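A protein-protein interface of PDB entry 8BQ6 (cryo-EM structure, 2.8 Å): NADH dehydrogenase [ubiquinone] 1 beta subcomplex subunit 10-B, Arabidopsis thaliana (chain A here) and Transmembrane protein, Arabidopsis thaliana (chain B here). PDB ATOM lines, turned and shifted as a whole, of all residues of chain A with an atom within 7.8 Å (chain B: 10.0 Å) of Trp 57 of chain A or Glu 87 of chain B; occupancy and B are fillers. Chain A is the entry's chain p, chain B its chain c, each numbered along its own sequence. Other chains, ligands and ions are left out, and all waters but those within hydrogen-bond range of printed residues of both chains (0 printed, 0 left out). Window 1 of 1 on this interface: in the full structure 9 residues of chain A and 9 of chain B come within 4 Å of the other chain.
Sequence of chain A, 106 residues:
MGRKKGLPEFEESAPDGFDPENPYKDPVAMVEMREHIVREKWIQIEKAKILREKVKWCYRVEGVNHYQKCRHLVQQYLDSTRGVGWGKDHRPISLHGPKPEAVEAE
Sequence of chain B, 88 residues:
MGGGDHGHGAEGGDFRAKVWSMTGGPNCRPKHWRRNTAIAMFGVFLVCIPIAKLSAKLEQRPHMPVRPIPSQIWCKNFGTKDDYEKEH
Printed residues of chain B within 4 Å of Ile 50 of chain A: Glu 87 (3.4 Å) and His 88 (3.8 Å). Of the printed residues of chain B, Glu 53 of chain A touches Glu 87 and His 88. Lys 56 of chain A touches none of the printed residues of chain B. Of the printed residues of chain B, Trp 57 of chain A touches Gln 60 (3.96 Å), Pro 62 (3.98 Å), Lys 81 (3.7 Å) and Glu 87 (3.3 Å). Of chain B, only Tyr 84 (3.6 Å) comes within 4 Å of Cys 58 of chain A. No residue of chain B comes within 4 Å of Arg 60 of chain A. Of chain B, only Pro 62, His 63 and Lys 81 come within 4 Å of Val 61 of chain A. Printed residues of chain A within 4 Å of Pro 62 of chain B: Trp 57 (3.98 Å) and Val 61 (3.8 Å). Of the printed residues of chain A, Tyr 84 of chain B touches Lys 54 (3.5 Å), Cys 58 (3.6 Å), Glu 62 (3.0 Å) and Leu 73 (3.97 Å). Printed residues of chain A within 4 Å of Lys 86 of chain B: Lys 54 (3.8 Å). Glu 87 of chain B touches just these residues of chain A: Ile 50 (3.4 Å), Glu 53 (3.6 Å), Lys 54 (2.9 Å) and Trp 57 (3.3 Å). The nearest printed residue of chain B that does not touch Trp 57 of chain A is Tyr 84 of chain B (4.1 Å). The nearest residue of chain A that does not touch Glu 87 of chain B is Leu 51 of chain A (5.5 Å).
O of Glu 87 of chain B lies close to O of Ile 50 of chain A (3.4 Å). NZ of Lys 54 of chain A is in hydrogen-bond range of O of Glu 87 of chain B (2.9 Å). A ring nitrogen (NE2) of His 63 of chain B lies within hydrogen-bond range of the backbone carbonyl oxygen (O) of Val 61 of chain A (3.0 Å). The backbone carbonyl oxygen of His 88 of chain B sits close to the side-chain carboxylate of Glu 53 of chain A, at 3.5 Å. The side-chain hydroxyl (OH) of Tyr 84 of chain B lies within hydrogen-bond range of the side-chain carboxylate (OE2) of Glu 62 of chain A (3.0 Å).
CB of His 88 of chain B touches CG2 of Ile 50 of chain A, at 3.8 Å. Glu 87 of chain B touches Glu 53 of chain A. Tyr 84 of chain B touches Lys 54 of chain A. NZ of Lys 54 of chain A touches O of Glu 85 of chain B, at 3.8 Å. Lys 54 of chain A touches Lys 86 of chain B (NZ to C, 3.8 Å). Gln 60 of chain B touches Trp 57 of chain A (CB to CH2, 3.96 Å). Pro 62 of chain B touches Trp 57 of chain A. Glu 87 of chain B touches Trp 57 of chain A. Lys 81 of chain B touches Val 61 of chain A (O to CG2, 3.3 Å). Tyr 84 of chain B touches Leu 73 of chain A.
Of the 17 printed residues of chain A, 8 touch a printed residue of chain B. Among the printed residues, 18 pairs touch across the chains.
The side-chain carboxylate (OD2) of Asp 83 of chain B lies within salt-bridge range of the side-chain amino group (NZ) of Lys 86 of chain B. The side-chain carboxylate (OE2) of Glu 53 of chain A sits at hydrogen-bond distance from the indole nitrogen (NE1) of Trp 57 of chain A. The side-chain sulfur (SG) of Cys 58 of chain A is disulfide-bonded to the side-chain sulfur (SG) of Cys 70 of chain A, 2.0 Å away. OE1 of Glu 87 of chain B lies within salt-bridge range of NZ of Lys 81 of chain B. The side-chain carboxylate (OE2) of Glu 53 of chain A is in salt-bridge range of the side-chain amino group (NZ) of Lys 56 of chain A (3.8 Å).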
ATOM      1  N   LYS A  49      20.985 -39.250  16.057  1.00  0.00           N
ATOM      2  CA  LYS A  49      21.621 -38.229  16.883  1.00  0.00           C
ATOM      3  C   LYS A  49      22.541 -37.340  16.057  1.00  0.00           C
ATOM      4  O   LYS A  49      22.655 -36.139  16.325  1.00  0.00           O
ATOM      5  CB  LYS A  49      22.383 -38.886  18.030  1.00  0.00           C
ATOM      6  CG  LYS A  49      21.476 -39.610  19.013  1.00  0.00           C
ATOM      7  CD  LYS A  49      22.107 -40.885  19.528  1.00  0.00           C
ATOM      8  CE  LYS A  49      23.311 -40.597  20.390  1.00  0.00           C
ATOM      9  NZ  LYS A  49      23.130 -39.364  21.189  1.00  0.00           N
ATOM     10  N   ILE A  50      23.185 -37.931  15.043  1.00  0.00           N
ATOM     11  CA  ILE A  50      24.023 -37.132  14.099  1.00  0.00           C
ATOM     12  C   ILE A  50      23.060 -36.247  13.304  1.00  0.00           C
ATOM     13  O   ILE A  50      23.346 -35.040  13.159  1.00  0.00           O
ATOM     14  CB  ILE A  50      24.837 -38.075  13.188  1.00  0.00           C
ATOM     15  CG1 ILE A  50      26.020 -38.700  13.931  1.00  0.00           C
ATOM     16  CG2 ILE A  50      25.286 -37.383  11.907  1.00  0.00           C
ATOM     17  CD1 ILE A  50      26.556 -39.954  13.281  1.00  0.00           C
ATOM     18  N   LEU A  51      21.946 -36.824  12.841  1.00  0.00           N
ATOM     19  CA  LEU A  51      20.953 -36.055  12.101  1.00  0.00           C
ATOM     20  C   LEU A  51      20.312 -34.991  12.978  1.00  0.00           C
ATOM     21  O   LEU A  51      19.869 -33.954  12.474  1.00  0.00           O
ATOM     22  CB  LEU A  51      19.880 -36.990  11.546  1.00  0.00           C
ATOM     23  CG  LEU A  51      20.283 -37.881  10.372  1.00  0.00           C
ATOM     24  CD1 LEU A  51      19.051 -38.438   9.692  1.00  0.00           C
ATOM     25  CD2 LEU A  51      21.159 -37.131   9.380  1.00  0.00           C
ATOM     26  N   ARG A  52      20.243 -35.234  14.287  1.00  0.00           N
ATOM     27  CA  ARG A  52      19.627 -34.265  15.185  1.00  0.00           C
ATOM     28  C   ARG A  52      20.543 -33.071  15.414  1.00  0.00           C
ATOM     29  O   ARG A  52      20.072 -31.935  15.543  1.00  0.00           O
ATOM     30  CB  ARG A  52      19.263 -34.945  16.501  1.00  0.00           C
ATOM     31  CG  ARG A  52      18.835 -34.011  17.603  1.00  0.00           C
ATOM     32  CD  ARG A  52      18.260 -34.808  18.750  1.00  0.00           C
ATOM     33  NE  ARG A  52      19.278 -35.578  19.451  1.00  0.00           N
ATOM     34  CZ  ARG A  52      19.022 -36.653  20.181  1.00  0.00           C
ATOM     35  NH1 ARG A  52      17.800 -37.152  20.270  1.00  0.00           N
ATOM     36  NH2 ARG A  52      20.014 -37.241  20.841  1.00  0.00           N
ATOM     37  N   GLU A  53      21.856 -33.318  15.415  1.00  0.00           N
ATOM     38  CA  GLU A  53      22.834 -32.206  15.550  1.00  0.00           C
ATOM     39  C   GLU A  53      22.699 -31.265  14.349  1.00  0.00           C
ATOM     40  O   GLU A  53      22.896 -30.049  14.533  1.00  0.00           O
ATOM     41  CB  GLU A  53      24.251 -32.767  15.637  1.00  0.00           C
ATOM     42  CG  GLU A  53      24.875 -32.599  17.005  1.00  0.00           C
ATOM     43  CD  GLU A  53      25.519 -31.242  17.222  1.00  0.00           C
ATOM     44  OE1 GLU A  53      26.494 -30.931  16.510  1.00  0.00           O
ATOM     45  OE2 GLU A  53      25.041 -30.500  18.102  1.00  0.00           O
ATOM     46  N   LYS A  54      22.375 -31.807  13.169  1.00  0.00           N
ATOM     47  CA  LYS A  54      22.208 -30.986  11.973  1.00  0.00           C
ATOM     48  C   LYS A  54      20.997 -30.070  12.095  1.00  0.00           C
ATOM     49  O   LYS A  54      21.066 -28.882  11.761  1.00  0.00           O
ATOM     50  CB  LYS A  54      22.075 -31.887  10.752  1.00  0.00           C
ATOM     51  CG  LYS A  54      23.344 -32.610  10.399  1.00  0.00           C
ATOM     52  CD  LYS A  54      23.156 -33.400   9.131  1.00  0.00           C
ATOM     53  CE  LYS A  54      24.026 -34.631   9.132  1.00  0.00           C
ATOM     54  NZ  LYS A  54      25.420 -34.283   9.503  1.00  0.00           N
ATOM     55  N   VAL A  55      19.874 -30.614  12.568  1.00  0.00           N
ATOM     56  CA  VAL A  55      18.668 -29.809  12.749  1.00  0.00           C
ATOM     57  C   VAL A  55      18.914 -28.712  13.771  1.00  0.00           C
ATOM     58  O   VAL A  55      18.467 -27.570  13.607  1.00  0.00           O
ATOM     59  CB  VAL A  55      17.483 -30.702  13.156  1.00  0.00           C
ATOM     60  CG1 VAL A  55      16.318 -29.857  13.629  1.00  0.00           C
ATOM     61  CG2 VAL A  55      17.055 -31.561  11.992  1.00  0.00           C
ATOM     62  N   LYS A  56      19.629 -29.045  14.844  1.00  0.00           N
ATOM     63  CA  LYS A  56      19.883 -28.074  15.898  1.00  0.00           C
ATOM     64  C   LYS A  56      20.605 -26.850  15.356  1.00  0.00           C
ATOM     65  O   LYS A  56      20.169 -25.712  15.558  1.00  0.00           O
ATOM     66  CB  LYS A  56      20.702 -28.722  17.009  1.00  0.00           C
ATOM     67  CG  LYS A  56      21.293 -27.723  17.972  1.00  0.00           C
ATOM     68  CD  LYS A  56      22.187 -28.408  18.979  1.00  0.00           C
ATOM     69  CE  LYS A  56      21.609 -29.738  19.416  1.00  0.00           C
ATOM     70  NZ  LYS A  56      22.240 -30.195  20.681  1.00  0.00           N
ATOM     71  N   TRP A  57      21.707 -27.068  14.643  1.00  0.00           N
ATOM     72  CA  TRP A  57      22.527 -25.936  14.229  1.00  0.00           C
ATOM     73  C   TRP A  57      21.899 -25.187  13.059  1.00  0.00           C
ATOM     74  O   TRP A  57      22.178 -24.000  12.869  1.00  0.00           O
ATOM     75  CB  TRP A  57      23.943 -26.409  13.912  1.00  0.00           C
ATOM     76  CG  TRP A  57      24.721 -26.659  15.165  1.00  0.00           C
ATOM     77  CD1 TRP A  57      25.164 -27.859  15.626  1.00  0.00           C
ATOM     78  CD2 TRP A  57      25.131 -25.682  16.131  1.00  0.00           C
ATOM     79  NE1 TRP A  57      25.830 -27.695  16.814  1.00  0.00           N
ATOM     80  CE2 TRP A  57      25.824 -26.367  17.147  1.00  0.00           C
ATOM     81  CE3 TRP A  57      24.986 -24.296  16.232  1.00  0.00           C
ATOM     82  CZ2 TRP A  57      26.368 -25.714  18.249  1.00  0.00           C
ATOM     83  CZ3 TRP A  57      25.527 -23.650  17.328  1.00  0.00           C
ATOM     84  CH2 TRP A  57      26.208 -24.359  18.321  1.00  0.00           C
ATOM     85  N   CYS A  58      21.053 -25.858  12.286  1.00  0.00           N
ATOM     86  CA  CYS A  58      20.305 -25.128  11.232  1.00  0.00           C
ATOM     87  C   CYS A  58      19.355 -24.131  11.908  1.00  0.00           C
ATOM     88  O   CYS A  58      19.336 -22.980  11.475  1.00  0.00           O
ATOM     89  CB  CYS A  58      19.531 -26.102  10.356  1.00  0.00           C
ATOM     90  SG  CYS A  58      18.866 -25.354   8.847  1.00  0.00           S
ATOM     91  N   TYR A  59      18.602 -24.547  12.933  1.00  0.00           N
ATOM     92  CA  TYR A  59      17.730 -23.635  13.666  1.00  0.00           C
ATOM     93  C   TYR A  59      18.535 -22.485  14.251  1.00  0.00           C
ATOM     94  O   TYR A  59      18.121 -21.322  14.209  1.00  0.00           O
ATOM     95  CB  TYR A  59      16.996 -24.396  14.777  1.00  0.00           C
ATOM     96  CG  TYR A  59      15.925 -23.607  15.509  1.00  0.00           C
ATOM     97  CD1 TYR A  59      14.606 -23.622  15.084  1.00  0.00           C
ATOM     98  CD2 TYR A  59      16.239 -22.850  16.630  1.00  0.00           C
ATOM     99  CE1 TYR A  59      13.630 -22.910  15.756  1.00  0.00           C
ATOM    100  CE2 TYR A  59      15.271 -22.136  17.303  1.00  0.00           C
ATOM    101  CZ  TYR A  59      13.971 -22.167  16.862  1.00  0.00           C
ATOM    102  OH  TYR A  59      13.009 -21.452  17.536  1.00  0.00           O
ATOM    103  N   ARG A  60      19.704 -22.803  14.807  1.00  0.00           N
ATOM    104  CA  ARG A  60      20.514 -21.779  15.452  1.00  0.00           C
ATOM    105  C   ARG A  60      21.123 -20.831  14.430  1.00  0.00           C
ATOM    106  O   ARG A  60      21.231 -19.626  14.679  1.00  0.00           O
ATOM    107  CB  ARG A  60      21.589 -22.443  16.305  1.00  0.00           C
ATOM    108  CG  ARG A  60      20.991 -23.308  17.391  1.00  0.00           C
ATOM    109  CD  ARG A  60      22.030 -24.062  18.171  1.00  0.00           C
ATOM    110  NE  ARG A  60      21.472 -24.518  19.437  1.00  0.00           N
ATOM    111  CZ  ARG A  60      22.181 -25.046  20.422  1.00  0.00           C
ATOM    112  NH1 ARG A  60      23.487 -25.227  20.313  1.00  0.00           N
ATOM    113  NH2 ARG A  60      21.567 -25.397  21.546  1.00  0.00           N
ATOM    114  N   VAL A  61      21.496 -21.351  13.261  1.00  0.00           N
ATOM    115  CA  VAL A  61      22.181 -20.544  12.256  1.00  0.00           C
ATOM    116  C   VAL A  61      21.192 -19.728  11.432  1.00  0.00           C
ATOM    117  O   VAL A  61      21.468 -18.575  11.082  1.00  0.00           O
ATOM    118  CB  VAL A  61      23.051 -21.452  11.369  1.00  0.00           C
ATOM    119  CG1 VAL A  61      23.340 -20.796  10.031  1.00  0.00           C
ATOM    120  CG2 VAL A  61      24.337 -21.786  12.089  1.00  0.00           C
ATOM    121  N   GLU A  62      20.046 -20.323  11.083  1.00  0.00           N
ATOM    122  CA  GLU A  62      19.088 -19.668  10.146  1.00  0.00           C
ATOM    123  C   GLU A  62      18.005 -18.832  10.838  1.00  0.00           C
ATOM    124  O   GLU A  62      17.430 -17.980  10.142  1.00  0.00           O
ATOM    125  CB  GLU A  62      18.475 -20.716   9.218  1.00  0.00           C
ATOM    126  CG  GLU A  62      19.514 -21.561   8.500  1.00  0.00           C
ATOM    127  CD  GLU A  62      20.256 -20.929   7.332  1.00  0.00           C
ATOM    128  OE1 GLU A  62      20.742 -19.790   7.465  1.00  0.00           O
ATOM    129  OE2 GLU A  62      20.370 -21.594   6.292  1.00  0.00           O
ATOM    130  N   GLY A  63      17.705 -19.061  12.117  1.00  0.00           N
ATOM    131  CA  GLY A  63      16.767 -18.191  12.803  1.00  0.00           C
ATOM    132  C   GLY A  63      15.383 -18.248  12.190  1.00  0.00           C
ATOM    133  O   GLY A  63      14.820 -19.323  11.963  1.00  0.00           O
ATOM    134  N   CYS A  70      15.568 -25.507   6.620  1.00  0.00           N
ATOM    135  CA  CYS A  70      15.880 -26.832   7.224  1.00  0.00           C
ATOM    136  C   CYS A  70      14.746 -27.829   6.966  1.00  0.00           C
ATOM    137  O   CYS A  70      14.830 -28.933   7.518  1.00  0.00           O
ATOM    138  CB  CYS A  70      16.165 -26.725   8.717  1.00  0.00           C
ATOM    139  SG  CYS A  70      16.895 -25.148   9.231  1.00  0.00           S
ATOM    140  N   LEU A  73      16.182 -31.169   6.395  1.00  0.00           N
ATOM    141  CA  LEU A  73      16.841 -31.841   7.515  1.00  0.00           C
ATOM    142  C   LEU A  73      15.832 -32.338   8.542  1.00  0.00           C
ATOM    143  O   LEU A  73      16.034 -33.391   9.159  1.00  0.00           O
ATOM    144  CB  LEU A  73      17.851 -30.909   8.183  1.00  0.00           C
ATOM    145  CG  LEU A  73      19.202 -30.695   7.506  1.00  0.00           C
ATOM    146  CD1 LEU A  73      20.103 -29.853   8.385  1.00  0.00           C
ATOM    147  CD2 LEU A  73      19.861 -32.020   7.172  1.00  0.00           C
ATOM    148  N   LEU B  58      34.420 -22.459  25.210  1.00  0.00           N
ATOM    149  CA  LEU B  58      33.219 -23.231  24.922  1.00  0.00           C
ATOM    150  C   LEU B  58      32.146 -22.450  24.173  1.00  0.00           C
ATOM    151  O   LEU B  58      31.290 -23.072  23.533  1.00  0.00           O
ATOM    152  CB  LEU B  58      32.625 -23.767  26.228  1.00  0.00           C
ATOM    153  CG  LEU B  58      32.795 -25.252  26.544  1.00  0.00           C
ATOM    154  CD1 LEU B  58      34.227 -25.691  26.331  1.00  0.00           C
ATOM    155  CD2 LEU B  58      32.367 -25.519  27.971  1.00  0.00           C
ATOM    156  N   GLU B  59      32.165 -21.119  24.225  1.00  0.00           N
ATOM    157  CA  GLU B  59      31.090 -20.344  23.619  1.00  0.00           C
ATOM    158  C   GLU B  59      31.059 -20.551  22.111  1.00  0.00           C
ATOM    159  O   GLU B  59      32.093 -20.765  21.473  1.00  0.00           O
ATOM    160  CB  GLU B  59      31.244 -18.854  23.926  1.00  0.00           C
ATOM    161  CG  GLU B  59      31.189 -18.485  25.391  1.00  0.00           C
ATOM    162  CD  GLU B  59      32.280 -17.506  25.777  1.00  0.00           C
ATOM    163  OE1 GLU B  59      33.286 -17.423  25.048  1.00  0.00           O
ATOM    164  OE2 GLU B  59      32.139 -16.831  26.814  1.00  0.00           O
ATOM    165  N   GLN B  60      29.855 -20.500  21.545  1.00  0.00           N
ATOM    166  CA  GLN B  60      29.648 -20.636  20.109  1.00  0.00           C
ATOM    167  C   GLN B  60      28.742 -19.509  19.648  1.00  0.00           C
ATOM    168  O   GLN B  60      27.605 -19.394  20.114  1.00  0.00           O
ATOM    169  CB  GLN B  60      29.038 -21.994  19.760  1.00  0.00           C
ATOM    170  CG  GLN B  60      29.907 -23.168  20.145  1.00  0.00           C
ATOM    171  CD  GLN B  60      30.940 -23.493  19.090  1.00  0.00           C
ATOM    172  OE1 GLN B  60      30.891 -22.970  17.979  1.00  0.00           O
ATOM    173  NE2 GLN B  60      31.877 -24.368  19.428  1.00  0.00           N
ATOM    174  N   ARG B  61      29.273 -18.645  18.776  1.00  0.00           N
ATOM    175  CA  ARG B  61      28.483 -17.492  18.264  1.00  0.00           C
ATOM    176  C   ARG B  61      28.362 -17.629  16.744  1.00  0.00           C
ATOM    177  O   ARG B  61      29.250 -17.129  16.036  1.00  0.00           O
ATOM    178  CB  ARG B  61      29.135 -16.162  18.655  1.00  0.00           C
ATOM    179  CG  ARG B  61      29.850 -16.173  19.998  1.00  0.00           C
ATOM    180  CD  ARG B  61      28.918 -15.895  21.160  1.00  0.00           C
ATOM    181  NE  ARG B  61      28.128 -14.679  21.022  1.00  0.00           N
ATOM    182  CZ  ARG B  61      28.272 -13.600  21.784  1.00  0.00           C
ATOM    183  NH1 ARG B  61      29.184 -13.580  22.740  1.00  0.00           N
ATOM    184  NH2 ARG B  61      27.504 -12.543  21.590  1.00  0.00           N
ATOM    185  N   PRO B  62      27.296 -18.264  16.208  1.00  0.00           N
ATOM    186  CA  PRO B  62      27.175 -18.509  14.765  1.00  0.00           C
ATOM    187  C   PRO B  62      26.960 -17.248  13.955  1.00  0.00           C
ATOM    188  O   PRO B  62      26.971 -17.317  12.721  1.00  0.00           O
ATOM    189  CB  PRO B  62      25.963 -19.449  14.666  1.00  0.00           C
ATOM    190  CG  PRO B  62      25.659 -19.869  16.086  1.00  0.00           C
ATOM    191  CD  PRO B  62      26.111 -18.738  16.937  1.00  0.00           C
ATOM    192  N   HIS B  63      26.760 -16.124  14.634  1.00  0.00           N
ATOM    193  CA  HIS B  63      26.417 -14.872  13.931  1.00  0.00           C
ATOM    194  C   HIS B  63      27.384 -13.752  14.285  1.00  0.00           C
ATOM    195  O   HIS B  63      27.626 -13.533  15.490  1.00  0.00           O
ATOM    196  CB  HIS B  63      24.996 -14.470  14.317  1.00  0.00           C
ATOM    197  CG  HIS B  63      23.949 -15.146  13.507  1.00  0.00           C
ATOM    198  ND1 HIS B  63      24.144 -15.465  12.181  1.00  0.00           N
ATOM    199  CD2 HIS B  63      22.707 -15.565  13.827  1.00  0.00           C
ATOM    200  CE1 HIS B  63      23.063 -16.047  11.713  1.00  0.00           C
ATOM    201  NE2 HIS B  63      22.167 -16.120  12.703  1.00  0.00           N
ATOM    202  N   ASN B  77      35.147 -18.237  18.098  1.00  0.00           N
ATOM    203  CA  ASN B  77      34.160 -19.166  17.557  1.00  0.00           C
ATOM    204  C   ASN B  77      33.030 -18.425  16.856  1.00  0.00           C
ATOM    205  O   ASN B  77      31.867 -18.832  16.911  1.00  0.00           O
ATOM    206  CB  ASN B  77      33.611 -20.069  18.654  1.00  0.00           C
ATOM    207  CG  ASN B  77      34.648 -21.028  19.182  1.00  0.00           C
ATOM    208  OD1 ASN B  77      35.151 -21.883  18.454  1.00  0.00           O
ATOM    209  ND2 ASN B  77      34.995 -20.877  20.451  1.00  0.00           N
ATOM    210  N   GLY B  79      30.989 -17.101  13.654  1.00  0.00           N
ATOM    211  CA  GLY B  79      30.712 -17.525  12.296  1.00  0.00           C
ATOM    212  C   GLY B  79      31.342 -18.856  11.945  1.00  0.00           C
ATOM    213  O   GLY B  79      31.981 -18.988  10.897  1.00  0.00           O
ATOM    214  N   THR B  80      31.186 -19.853  12.814  1.00  0.00           N
ATOM    215  CA  THR B  80      31.786 -21.156  12.576  1.00  0.00           C
ATOM    216  C   THR B  80      30.777 -22.230  12.192  1.00  0.00           C
ATOM    217  O   THR B  80      31.132 -23.153  11.452  1.00  0.00           O
ATOM    218  CB  THR B  80      32.577 -21.599  13.817  1.00  0.00           C
ATOM    219  OG1 THR B  80      33.660 -20.687  14.027  1.00  0.00           O
ATOM    220  CG2 THR B  80      33.146 -23.001  13.650  1.00  0.00           C
ATOM    221  N   LYS B  81      29.537 -22.142  12.666  1.00  0.00           N
ATOM    222  CA  LYS B  81      28.599 -23.271  12.411  1.00  0.00           C
ATOM    223  C   LYS B  81      27.837 -23.049  11.100  1.00  0.00           C
ATOM    224  O   LYS B  81      26.761 -23.656  10.948  1.00  0.00           O
ATOM    225  CB  LYS B  81      27.689 -23.486  13.626  1.00  0.00           C
ATOM    226  CG  LYS B  81      28.411 -23.602  14.963  1.00  0.00           C
ATOM    227  CD  LYS B  81      29.507 -24.643  14.970  1.00  0.00           C
ATOM    228  CE  LYS B  81      29.428 -25.588  16.148  1.00  0.00           C
ATOM    229  NZ  LYS B  81      30.118 -26.866  15.866  1.00  0.00           N
ATOM    230  N   ASP B  82      28.404 -22.272  10.170  1.00  0.00           N
ATOM    231  CA  ASP B  82      27.768 -22.054   8.843  1.00  0.00           C
ATOM    232  C   ASP B  82      27.496 -23.407   8.177  1.00  0.00           C
ATOM    233  O   ASP B  82      26.359 -23.612   7.720  1.00  0.00           O
ATOM    234  CB  ASP B  82      28.632 -21.164   7.949  1.00  0.00           C
ATOM    235  CG  ASP B  82      28.324 -19.682   8.105  1.00  0.00           C
ATOM    236  OD1 ASP B  82      27.313 -19.355   8.764  1.00  0.00           O
ATOM    237  OD2 ASP B  82      29.095 -18.863   7.563  1.00  0.00           O
ATOM    238  N   ASP B  83      28.506 -24.284   8.119  1.00  0.00           N
ATOM    239  CA  ASP B  83      28.304 -25.640   7.548  1.00  0.00           C
ATOM    240  C   ASP B  83      27.514 -26.475   8.554  1.00  0.00           C
ATOM    241  O   ASP B  83      28.152 -27.123   9.411  1.00  0.00           O
ATOM    242  CB  ASP B  83      29.633 -26.292   7.158  1.00  0.00           C
ATOM    243  CG  ASP B  83      30.283 -25.658   5.941  1.00  0.00           C
ATOM    244  OD1 ASP B  83      29.591 -24.908   5.223  1.00  0.00           O
ATOM    245  OD2 ASP B  83      31.480 -25.920   5.720  1.00  0.00           O
ATOM    246  N   TYR B  84      26.183 -26.439   8.472  1.00  0.00           N
ATOM    247  CA  TYR B  84      25.348 -27.161   9.469  1.00  0.00           C
ATOM    248  C   TYR B  84      25.052 -28.583   8.976  1.00  0.00           C
ATOM    249  O   TYR B  84      24.766 -29.455   9.812  1.00  0.00           O
ATOM    250  CB  TYR B  84      24.085 -26.366   9.821  1.00  0.00           C
ATOM    251  CG  TYR B  84      23.243 -25.862   8.675  1.00  0.00           C
ATOM    252  CD1 TYR B  84      22.508 -26.729   7.883  1.00  0.00           C
ATOM    253  CD2 TYR B  84      23.138 -24.507   8.418  1.00  0.00           C
ATOM    254  CE1 TYR B  84      21.730 -26.270   6.835  1.00  0.00           C
ATOM    255  CE2 TYR B  84      22.359 -24.029   7.379  1.00  0.00           C
ATOM    256  CZ  TYR B  84      21.649 -24.912   6.587  1.00  0.00           C
ATOM    257  OH  TYR B  84      20.871 -24.452   5.564  1.00  0.00           O
ATOM    258  N   GLU B  85      25.077 -28.793   7.659  1.00  0.00           N
ATOM    259  CA  GLU B  85      24.806 -30.136   7.079  1.00  0.00           C
ATOM    260  C   GLU B  85      26.050 -31.015   7.232  1.00  0.00           C
ATOM    261  O   GLU B  85      26.123 -32.042   6.534  1.00  0.00           O
ATOM    262  CB  GLU B  85      24.397 -29.989   5.613  1.00  0.00           C
ATOM    263  CG  GLU B  85      23.060 -29.294   5.437  1.00  0.00           C
ATOM    264  CD  GLU B  85      22.647 -29.061   3.994  1.00  0.00           C
ATOM    265  OE1 GLU B  85      23.484 -29.269   3.094  1.00  0.00           O
ATOM    266  OE2 GLU B  85      21.484 -28.675   3.772  1.00  0.00           O
ATOM    267  N   LYS B  86      26.932 -30.665   8.175  1.00  0.00           N
ATOM    268  CA  LYS B  86      28.146 -31.471   8.461  1.00  0.00           C
ATOM    269  C   LYS B  86      28.209 -31.781   9.963  1.00  0.00           C
ATOM    270  O   LYS B  86      29.025 -32.645  10.341  1.00  0.00           O
ATOM    271  CB  LYS B  86      29.394 -30.693   8.038  1.00  0.00           C
ATOM    272  CG  LYS B  86      29.550 -30.466   6.542  1.00  0.00           C
ATOM    273  CD  LYS B  86      30.787 -29.672   6.184  1.00  0.00           C
ATOM    274  CE  LYS B  86      30.953 -29.467   4.693  1.00  0.00           C
ATOM    275  NZ  LYS B  86      32.161 -28.666   4.380  1.00  0.00           N
ATOM    276  N   GLU B  87      27.382 -31.115  10.779  1.00  0.00           N
ATOM    277  CA  GLU B  87      27.418 -31.292  12.260  1.00  0.00           C
ATOM    278  C   GLU B  87      27.028 -32.722  12.651  1.00  0.00           C
ATOM    279  O   GLU B  87      26.023 -33.229  12.124  1.00  0.00           O
ATOM    280  CB  GLU B  87      26.480 -30.290  12.936  1.00  0.00           C
ATOM    281  CG  GLU B  87      26.733 -28.853  12.520  1.00  0.00           C
ATOM    282  CD  GLU B  87      27.872 -28.147  13.234  1.00  0.00           C
ATOM    283  OE1 GLU B  87      28.193 -28.541  14.373  1.00  0.00           O
ATOM    284  OE2 GLU B  87      28.430 -27.198  12.651  1.00  0.00           O
ATOM    285  N   HIS B  88      27.786 -33.329  13.569  1.00  0.00           N
ATOM    286  CA  HIS B  88      27.495 -34.720  14.016  1.00  0.00           C
ATOM    287  C   HIS B  88      27.549 -34.818  15.547  1.00  0.00           C
ATOM    288  O   HIS B  88      28.207 -33.954  16.164  1.00  0.00           O
ATOM    289  CB  HIS B  88      28.441 -35.712  13.326  1.00  0.00           C
ATOM    290  CG  HIS B  88      29.884 -35.505  13.641  1.00  0.00           C
ATOM    291  ND1 HIS B  88      30.522 -36.192  14.654  1.00  0.00           N
ATOM    292  CD2 HIS B  88      30.816 -34.707  13.077  1.00  0.00           C
ATOM    293  CE1 HIS B  88      31.784 -35.820  14.708  1.00  0.00           C
ATOM    294  NE2 HIS B  88      31.990 -34.909  13.750  1.00  0.00           N
